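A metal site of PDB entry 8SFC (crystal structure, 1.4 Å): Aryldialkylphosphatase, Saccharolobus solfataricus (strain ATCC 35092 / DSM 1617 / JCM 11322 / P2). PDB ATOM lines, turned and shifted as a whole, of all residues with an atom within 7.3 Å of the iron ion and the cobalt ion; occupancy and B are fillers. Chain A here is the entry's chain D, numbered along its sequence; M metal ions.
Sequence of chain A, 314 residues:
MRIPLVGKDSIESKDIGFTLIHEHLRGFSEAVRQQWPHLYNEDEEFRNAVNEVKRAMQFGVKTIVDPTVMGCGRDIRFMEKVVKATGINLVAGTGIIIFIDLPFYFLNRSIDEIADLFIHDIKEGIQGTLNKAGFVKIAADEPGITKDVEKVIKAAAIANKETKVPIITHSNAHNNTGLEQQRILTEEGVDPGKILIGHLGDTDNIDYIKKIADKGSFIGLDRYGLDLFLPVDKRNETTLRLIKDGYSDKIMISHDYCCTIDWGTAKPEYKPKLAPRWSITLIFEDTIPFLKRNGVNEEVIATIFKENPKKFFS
OG1 of Thr 260 lies close to SG of Cys 258 (3.1 Å). The backbone carbonyl oxygen (O) of Ile 138 is in hydrogen-bond range of the backbone NH (N) of His 170. The backbone NH (N) of His 199 lies within hydrogen-bond range of the side-chain carboxylate (OD1) of Asp 222 (2.8 Å). The side-chain carboxylate (OD1) of Asp 256 lies close to the backbone carbonyl oxygen (O) of Asp 222 (2.6 Å). The side-chain carboxylate of Asp 256 lies close to a ring nitrogen (NE2) of His 22. N of Cys 258 lies within hydrogen-bond range of OD2 of Asp 256 (3.3 Å). The side-chain carboxylate of Glu 23 sits at hydrogen-bond distance from the backbone NH of Asp 256 (3.0 Å). NE2 of His 170 is in hydrogen-bond range of OD1 of Asp 141 (2.8 Å).
Cys 259 touches the iron ion (N to FE, 3.7 Å). Of the 26 residues printed, 5 come within 4 Å of the iron ion. The nearest printed residue that does not touch the iron ion is Cys 258 (4.04 Å).
Within 4 Å of the cobalt ion: KCX 137, His 170, His 199 and Cys 258. Along chain A the residues within 4 Å of the cobalt ion span positions 137 to 258.
The iron ion is bound by OQ1 of KCX 137 (2.0 Å), a ring nitrogen (NE2) of His 24 (2.0 Å) and a ring nitrogen (NE2) of His 22 (2.3 Å). The iron ion has three donor atoms within binding distance. Slightly farther from the iron ion lies the side-chain carboxylate (OD2) of Asp 256 (2.7 Å).
The cobalt ion is bound by ND1 of His 170 (2.0 Å), NE2 of His 199 (2.2 Å), OQ2 of KCX 137 (2.5 Å) and SG of Cys 258 (2.6 Å).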
ATOM      1  N   HIS A  22      22.476  10.872  36.263  1.00  0.00           N
ATOM      2  CA  HIS A  22      23.449  11.591  35.440  1.00  0.00           C
ATOM      3  C   HIS A  22      23.085  13.069  35.416  1.00  0.00           C
ATOM      4  O   HIS A  22      22.415  13.510  34.488  1.00  0.00           O
ATOM      5  CB  HIS A  22      23.442  10.992  34.032  1.00  0.00           C
ATOM      6  CG  HIS A  22      24.577  11.445  33.163  1.00  0.00           C
ATOM      7  ND1 HIS A  22      25.475  10.566  32.597  1.00  0.00           N
ATOM      8  CD2 HIS A  22      24.967  12.683  32.769  1.00  0.00           C
ATOM      9  CE1 HIS A  22      26.367  11.248  31.890  1.00  0.00           C
ATOM     10  NE2 HIS A  22      26.076  12.533  31.973  1.00  0.00           N
ATOM     11  N   GLU A  23      23.480  13.819  36.446  1.00  0.00           N
ATOM     12  CA  GLU A  23      23.196  15.251  36.541  1.00  0.00           C
ATOM     13  C   GLU A  23      24.430  15.974  37.040  1.00  0.00           C
ATOM     14  O   GLU A  23      24.946  15.656  38.121  1.00  0.00           O
ATOM     15  CB  GLU A  23      22.063  15.526  37.533  1.00  0.00           C
ATOM     16  CG  GLU A  23      20.842  14.624  37.376  1.00  0.00           C
ATOM     17  CD  GLU A  23      20.048  14.910  36.114  1.00  0.00           C
ATOM     18  OE1 GLU A  23      20.226  15.967  35.496  1.00  0.00           O
ATOM     19  OE2 GLU A  23      19.214  14.048  35.751  1.00  0.00           O
ATOM     20  N   HIS A  24      24.851  17.006  36.322  1.00  0.00           N
ATOM     21  CA  HIS A  24      26.056  17.762  36.664  1.00  0.00           C
ATOM     22  C   HIS A  24      25.698  19.014  37.443  1.00  0.00           C
ATOM     23  O   HIS A  24      24.902  19.834  36.971  1.00  0.00           O
ATOM     24  CB  HIS A  24      26.801  18.167  35.392  1.00  0.00           C
ATOM     25  CG  HIS A  24      27.167  17.023  34.511  1.00  0.00           C
ATOM     26  ND1 HIS A  24      28.402  16.413  34.556  1.00  0.00           N
ATOM     27  CD2 HIS A  24      26.474  16.410  33.519  1.00  0.00           C
ATOM     28  CE1 HIS A  24      28.437  15.440  33.655  1.00  0.00           C
ATOM     29  NE2 HIS A  24      27.285  15.425  33.012  1.00  0.00           N
ATOM     30  N   PRO A  67      28.332  12.983  37.257  1.00  0.00           N
ATOM     31  CA  PRO A  67      29.477  12.349  36.579  1.00  0.00           C
ATOM     32  C   PRO A  67      30.491  13.339  36.028  1.00  0.00           C
ATOM     33  O   PRO A  67      31.130  13.061  34.998  1.00  0.00           O
ATOM     34  CB  PRO A  67      28.809  11.560  35.447  1.00  0.00           C
ATOM     35  CG  PRO A  67      27.653  12.432  35.054  1.00  0.00           C
ATOM     36  CD  PRO A  67      27.172  13.126  36.346  1.00  0.00           C
ATOM     37  N   THR A  68      30.629  14.488  36.685  1.00  0.00           N
ATOM     38  CA  THR A  68      31.633  15.467  36.304  1.00  0.00           C
ATOM     39  C   THR A  68      33.012  14.941  36.727  1.00  0.00           C
ATOM     40  O   THR A  68      33.232  14.632  37.905  1.00  0.00           O
ATOM     41  CB  THR A  68      31.357  16.789  37.017  1.00  0.00           C
ATOM     42  OG1 THR A  68      29.982  17.191  36.836  1.00  0.00           O
ATOM     43  CG2 THR A  68      32.254  17.909  36.497  1.00  0.00           C
ATOM     44  N   CYS A  72      35.800  18.213  32.641  1.00  0.00           N
ATOM     45  CA  CYS A  72      34.575  18.943  32.893  1.00  0.00           C
ATOM     46  C   CYS A  72      34.591  19.667  34.212  1.00  0.00           C
ATOM     47  O   CYS A  72      33.571  20.226  34.616  1.00  0.00           O
ATOM     48  CB  CYS A  72      33.365  18.004  32.830  1.00  0.00           C
ATOM     49  SG  CYS A  72      32.695  17.649  31.164  1.00  0.00           S
ATOM     50  N   ILE A  97      37.148  12.634  30.519  1.00  0.00           N
ATOM     51  CA  ILE A  97      36.355  12.855  29.308  1.00  0.00           C
ATOM     52  C   ILE A  97      37.266  13.482  28.264  1.00  0.00           C
ATOM     53  O   ILE A  97      37.702  14.628  28.393  1.00  0.00           O
ATOM     54  CB  ILE A  97      35.129  13.750  29.584  1.00  0.00           C
ATOM     55  CG1 ILE A  97      34.129  12.996  30.467  1.00  0.00           C
ATOM     56  CG2 ILE A  97      34.464  14.167  28.284  1.00  0.00           C
ATOM     57  CD1 ILE A  97      33.107  13.887  31.116  1.00  0.00           C
ATOM     58  N   PHE A  99      37.762  13.400  23.738  1.00  0.00           N
ATOM     59  CA  PHE A  99      37.252  12.941  22.457  1.00  0.00           C
ATOM     60  C   PHE A  99      38.349  12.543  21.476  1.00  0.00           C
ATOM     61  O   PHE A  99      38.068  11.776  20.540  1.00  0.00           O
ATOM     62  CB  PHE A  99      36.375  14.014  21.785  1.00  0.00           C
ATOM     63  CG  PHE A  99      35.078  14.325  22.510  1.00  0.00           C
ATOM     64  CD1 PHE A  99      34.664  13.586  23.612  1.00  0.00           C
ATOM     65  CD2 PHE A  99      34.287  15.368  22.070  1.00  0.00           C
ATOM     66  CE1 PHE A  99      33.471  13.893  24.261  1.00  0.00           C
ATOM     67  CE2 PHE A  99      33.105  15.683  22.716  1.00  0.00           C
ATOM     68  CZ  PHE A  99      32.701  14.939  23.809  1.00  0.00           C
ATOM     69  N   KCX A 137      33.728   7.442  34.956  1.00  0.00           N
ATOM     70  CA  KCX A 137      33.101   8.056  33.786  1.00  0.00           C
ATOM     71  CB  KCX A 137      32.501   9.413  34.179  1.00  0.00           C
ATOM     72  CG  KCX A 137      32.045  10.276  33.028  1.00  0.00           C
ATOM     73  CD  KCX A 137      30.776   9.717  32.390  1.00  0.00           C
ATOM     74  CE  KCX A 137      30.338  10.548  31.199  1.00  0.00           C
ATOM     75  NZ  KCX A 137      29.952  11.920  31.594  1.00  0.00           N
ATOM     76  C   KCX A 137      34.121   8.215  32.666  1.00  0.00           C
ATOM     77  O   KCX A 137      35.229   8.712  32.895  1.00  0.00           O
ATOM     78  CX  KCX A 137      29.251  12.742  30.815  1.00  0.00           C
ATOM     79  OQ1 KCX A 137      28.986  13.877  31.239  1.00  0.00           O
ATOM     80  OQ2 KCX A 137      28.882  12.417  29.681  1.00  0.00           O
ATOM     81  N   ILE A 138      33.753   7.790  31.457  1.00  0.00           N
ATOM     82  CA  ILE A 138      34.622   7.843  30.276  1.00  0.00           C
ATOM     83  C   ILE A 138      33.787   8.315  29.095  1.00  0.00           C
ATOM     84  O   ILE A 138      32.559   8.380  29.195  1.00  0.00           O
ATOM     85  CB  ILE A 138      35.255   6.468  29.978  1.00  0.00           C
ATOM     86  CG1 ILE A 138      34.170   5.450  29.631  1.00  0.00           C
ATOM     87  CG2 ILE A 138      36.110   5.998  31.169  1.00  0.00           C
ATOM     88  CD1 ILE A 138      34.704   4.084  29.320  1.00  0.00           C
ATOM     89  N   ALA A 139      34.439   8.599  27.965  1.00  0.00           N
ATOM     90  CA  ALA A 139      33.725   9.172  26.826  1.00  0.00           C
ATOM     91  C   ALA A 139      34.328   8.722  25.499  1.00  0.00           C
ATOM     92  O   ALA A 139      35.479   8.283  25.403  1.00  0.00           O
ATOM     93  CB  ALA A 139      33.788  10.701  26.852  1.00  0.00           C
ATOM     94  N   ASP A 141      33.285  10.253  21.171  1.00  0.00           N
ATOM     95  CA  ASP A 141      32.273  11.028  20.459  1.00  0.00           C
ATOM     96  C   ASP A 141      32.488  10.885  18.954  1.00  0.00           C
ATOM     97  O   ASP A 141      32.820   9.784  18.480  1.00  0.00           O
ATOM     98  CB  ASP A 141      32.320  12.500  20.894  1.00  0.00           C
ATOM     99  CG  ASP A 141      31.011  13.236  20.617  1.00  0.00           C
ATOM    100  OD1 ASP A 141      30.062  13.132  21.438  1.00  0.00           O
ATOM    101  OD2 ASP A 141      30.932  13.932  19.582  1.00  0.00           O
ATOM    102  N   ILE A 168      30.062   4.619  33.783  1.00  0.00           N
ATOM    103  CA  ILE A 168      29.137   5.422  33.014  1.00  0.00           C
ATOM    104  C   ILE A 168      29.893   5.957  31.814  1.00  0.00           C
ATOM    105  O   ILE A 168      31.038   6.387  31.953  1.00  0.00           O
ATOM    106  CB  ILE A 168      28.592   6.584  33.877  1.00  0.00           C
ATOM    107  CG1 ILE A 168      27.882   6.036  35.115  1.00  0.00           C
ATOM    108  CG2 ILE A 168      27.734   7.495  33.026  1.00  0.00           C
ATOM    109  CD1 ILE A 168      27.382   7.116  36.103  1.00  0.00           C
ATOM    110  N   THR A 169      29.263   5.959  30.634  1.00  0.00           N
ATOM    111  CA  THR A 169      29.911   6.525  29.466  1.00  0.00           C
ATOM    112  C   THR A 169      29.121   7.669  28.860  1.00  0.00           C
ATOM    113  O   THR A 169      27.895   7.756  28.984  1.00  0.00           O
ATOM    114  CB  THR A 169      30.169   5.484  28.364  1.00  0.00           C
ATOM    115  OG1 THR A 169      29.003   5.358  27.541  1.00  0.00           O
ATOM    116  CG2 THR A 169      30.515   4.158  28.967  1.00  0.00           C
ATOM    117  N   HIS A 170      29.864   8.552  28.206  1.00  0.00           N
ATOM    118  CA  HIS A 170      29.346   9.470  27.207  1.00  0.00           C
ATOM    119  C   HIS A 170      29.614   8.827  25.860  1.00  0.00           C
ATOM    120  O   HIS A 170      30.731   8.372  25.596  1.00  0.00           O
ATOM    121  CB  HIS A 170      30.107  10.786  27.301  1.00  0.00           C
ATOM    122  CG  HIS A 170      29.930  11.703  26.135  1.00  0.00           C
ATOM    123  ND1 HIS A 170      29.403  12.973  26.260  1.00  0.00           N
ATOM    124  CD2 HIS A 170      30.299  11.582  24.828  1.00  0.00           C
ATOM    125  CE1 HIS A 170      29.398  13.562  25.086  1.00  0.00           C
ATOM    126  NE2 HIS A 170      29.936  12.744  24.200  1.00  0.00           N
ATOM    127  N   SER A 171      28.589   8.780  25.012  1.00  0.00           N
ATOM    128  CA  SER A 171      28.779   8.313  23.642  1.00  0.00           C
ATOM    129  C   SER A 171      28.082   9.264  22.683  1.00  0.00           C
ATOM    130  O   SER A 171      27.312  10.145  23.094  1.00  0.00           O
ATOM    131  CB  SER A 171      28.290   6.866  23.440  1.00  0.00           C
ATOM    132  OG  SER A 171      26.889   6.811  23.267  1.00  0.00           O
ATOM    133  N   GLY A 198      25.711   6.057  27.734  1.00  0.00           N
ATOM    134  CA  GLY A 198      24.967   7.278  27.828  1.00  0.00           C
ATOM    135  C   GLY A 198      24.742   7.986  26.504  1.00  0.00           C
ATOM    136  O   GLY A 198      25.401   7.709  25.505  1.00  0.00           O
ATOM    137  N   HIS A 199      23.773   8.899  26.529  1.00  0.00           N
ATOM    138  CA  HIS A 199      23.493   9.833  25.444  1.00  0.00           C
ATOM    139  C   HIS A 199      22.773   9.177  24.274  1.00  0.00           C
ATOM    140  O   HIS A 199      22.750   9.725  23.174  1.00  0.00           O
ATOM    141  CB  HIS A 199      24.753  10.576  25.013  1.00  0.00           C
ATOM    142  CG  HIS A 199      25.277  11.476  26.074  1.00  0.00           C
ATOM    143  ND1 HIS A 199      24.677  11.587  27.312  1.00  0.00           N
ATOM    144  CD2 HIS A 199      26.379  12.271  26.126  1.00  0.00           C
ATOM    145  CE1 HIS A 199      25.360  12.436  28.065  1.00  0.00           C
ATOM    146  NE2 HIS A 199      26.392  12.859  27.364  1.00  0.00           N
ATOM    147  N   ASP A 222      19.253   9.887  28.476  1.00  0.00           N
ATOM    148  CA  ASP A 222      19.679  10.870  29.468  1.00  0.00           C
ATOM    149  C   ASP A 222      20.051  12.193  28.817  1.00  0.00           C
ATOM    150  O   ASP A 222      21.029  12.839  29.210  1.00  0.00           O
ATOM    151  CB  ASP A 222      20.822  10.312  30.312  1.00  0.00           C
ATOM    152  CG  ASP A 222      21.990   9.813  29.475  1.00  0.00           C
ATOM    153  OD1 ASP A 222      22.038  10.150  28.271  1.00  0.00           O
ATOM    154  OD2 ASP A 222      22.832   9.050  29.986  1.00  0.00           O
ATOM    155  N   ARG A 223      19.284  12.627  27.817  1.00  0.00           N
ATOM    156  CA  ARG A 223      19.492  13.933  27.197  1.00  0.00           C
ATOM    157  C   ARG A 223      18.241  14.799  27.300  1.00  0.00           C
ATOM    158  O   ARG A 223      18.156  15.839  26.637  1.00  0.00           O
ATOM    159  CB  ARG A 223      19.955  13.776  25.740  1.00  0.00           C
ATOM    160  CG  ARG A 223      20.365  15.049  25.013  1.00  0.00           C
ATOM    161  CD  ARG A 223      21.762  15.483  25.389  1.00  0.00           C
ATOM    162  NE  ARG A 223      22.767  14.638  24.763  1.00  0.00           N
ATOM    163  CZ  ARG A 223      24.072  14.797  24.890  1.00  0.00           C
ATOM    164  NH1 ARG A 223      24.582  15.733  25.683  1.00  0.00           N
ATOM    165  NH2 ARG A 223      24.895  14.008  24.207  1.00  0.00           N
ATOM    166  N   HIS A 255      18.574  14.262  32.558  1.00  0.00           N
ATOM    167  CA  HIS A 255      18.588  15.462  31.713  1.00  0.00           C
ATOM    168  C   HIS A 255      20.015  15.911  31.468  1.00  0.00           C
ATOM    169  O   HIS A 255      20.416  16.109  30.313  1.00  0.00           O
ATOM    170  CB  HIS A 255      17.973  16.661  32.440  1.00  0.00           C
ATOM    171  CG  HIS A 255      16.869  16.322  33.378  1.00  0.00           C
ATOM    172  ND1 HIS A 255      17.065  15.546  34.492  1.00  0.00           N
ATOM    173  CD2 HIS A 255      15.575  16.723  33.416  1.00  0.00           C
ATOM    174  CE1 HIS A 255      15.924  15.458  35.165  1.00  0.00           C
ATOM    175  NE2 HIS A 255      15.012  16.181  34.540  1.00  0.00           N
ATOM    176  N   ASP A 256      20.751  16.162  32.555  1.00  0.00           N
ATOM    177  CA  ASP A 256      22.118  16.646  32.613  1.00  0.00           C
ATOM    178  C   ASP A 256      22.440  17.756  31.619  1.00  0.00           C
ATOM    179  O   ASP A 256      22.943  18.810  32.009  1.00  0.00           O
ATOM    180  CB  ASP A 256      23.110  15.477  32.516  1.00  0.00           C
ATOM    181  CG  ASP A 256      23.462  15.088  31.099  1.00  0.00           C
ATOM    182  OD1 ASP A 256      22.644  14.412  30.443  1.00  0.00           O
ATOM    183  OD2 ASP A 256      24.596  15.369  30.657  1.00  0.00           O
ATOM    184  N   TYR A 257      22.121  17.540  30.349  1.00  0.00           N
ATOM    185  CA  TYR A 257      22.821  18.134  29.211  1.00  0.00           C
ATOM    186  C   TYR A 257      24.327  17.994  29.427  1.00  0.00           C
ATOM    187  O   TYR A 257      24.835  18.127  30.548  1.00  0.00           O
ATOM    188  CB  TYR A 257      22.365  19.565  28.880  1.00  0.00           C
ATOM    189  CG  TYR A 257      22.988  20.690  29.686  1.00  0.00           C
ATOM    190  CD1 TYR A 257      24.320  21.043  29.517  1.00  0.00           C
ATOM    191  CD2 TYR A 257      22.224  21.398  30.601  1.00  0.00           C
ATOM    192  CE1 TYR A 257      24.885  22.075  30.245  1.00  0.00           C
ATOM    193  CE2 TYR A 257      22.778  22.422  31.333  1.00  0.00           C
ATOM    194  CZ  TYR A 257      24.108  22.762  31.159  1.00  0.00           C
ATOM    195  OH  TYR A 257      24.652  23.787  31.890  1.00  0.00           O
ATOM    196  N   CYS A 258      25.050  17.717  28.351  1.00  0.00           N
ATOM    197  CA  CYS A 258      26.432  17.272  28.486  1.00  0.00           C
ATOM    198  C   CYS A 258      27.285  18.285  29.242  1.00  0.00           C
ATOM    199  O   CYS A 258      27.182  19.503  29.014  1.00  0.00           O
ATOM    200  CB  CYS A 258      27.003  17.044  27.104  1.00  0.00           C
ATOM    201  SG  CYS A 258      28.614  16.380  27.171  1.00  0.00           S
ATOM    202  N   CYS A 259      28.142  17.796  30.145  1.00  0.00           N
ATOM    203  CA  CYS A 259      28.990  18.692  30.932  1.00  0.00           C
ATOM    204  C   CYS A 259      30.025  19.409  30.076  1.00  0.00           C
ATOM    205  O   CYS A 259      30.571  20.424  30.516  1.00  0.00           O
ATOM    206  CB  CYS A 259      29.727  17.976  32.058  1.00  0.00           C
ATOM    207  SG  CYS A 259      30.908  16.696  31.528  1.00  0.00           S
ATOM    208  N   THR A 260      30.330  18.885  28.884  1.00  0.00           N
ATOM    209  CA  THR A 260      31.269  19.543  27.990  1.00  0.00           C
ATOM    210  C   THR A 260      30.739  20.870  27.454  1.00  0.00           C
ATOM    211  O   THR A 260      31.515  21.646  26.892  1.00  0.00           O
ATOM    212  CB  THR A 260      31.664  18.615  26.837  1.00  0.00           C
ATOM    213  OG1 THR A 260      30.552  18.425  25.965  1.00  0.00           O
ATOM    214  CG2 THR A 260      32.109  17.261  27.386  1.00  0.00           C
HETATM  215 FE    FE M   1      27.085  14.435  31.288  1.00  0.00          FE
HETATM  216 CO    CO M   2      28.320  13.839  27.721  1.00  0.00          CO
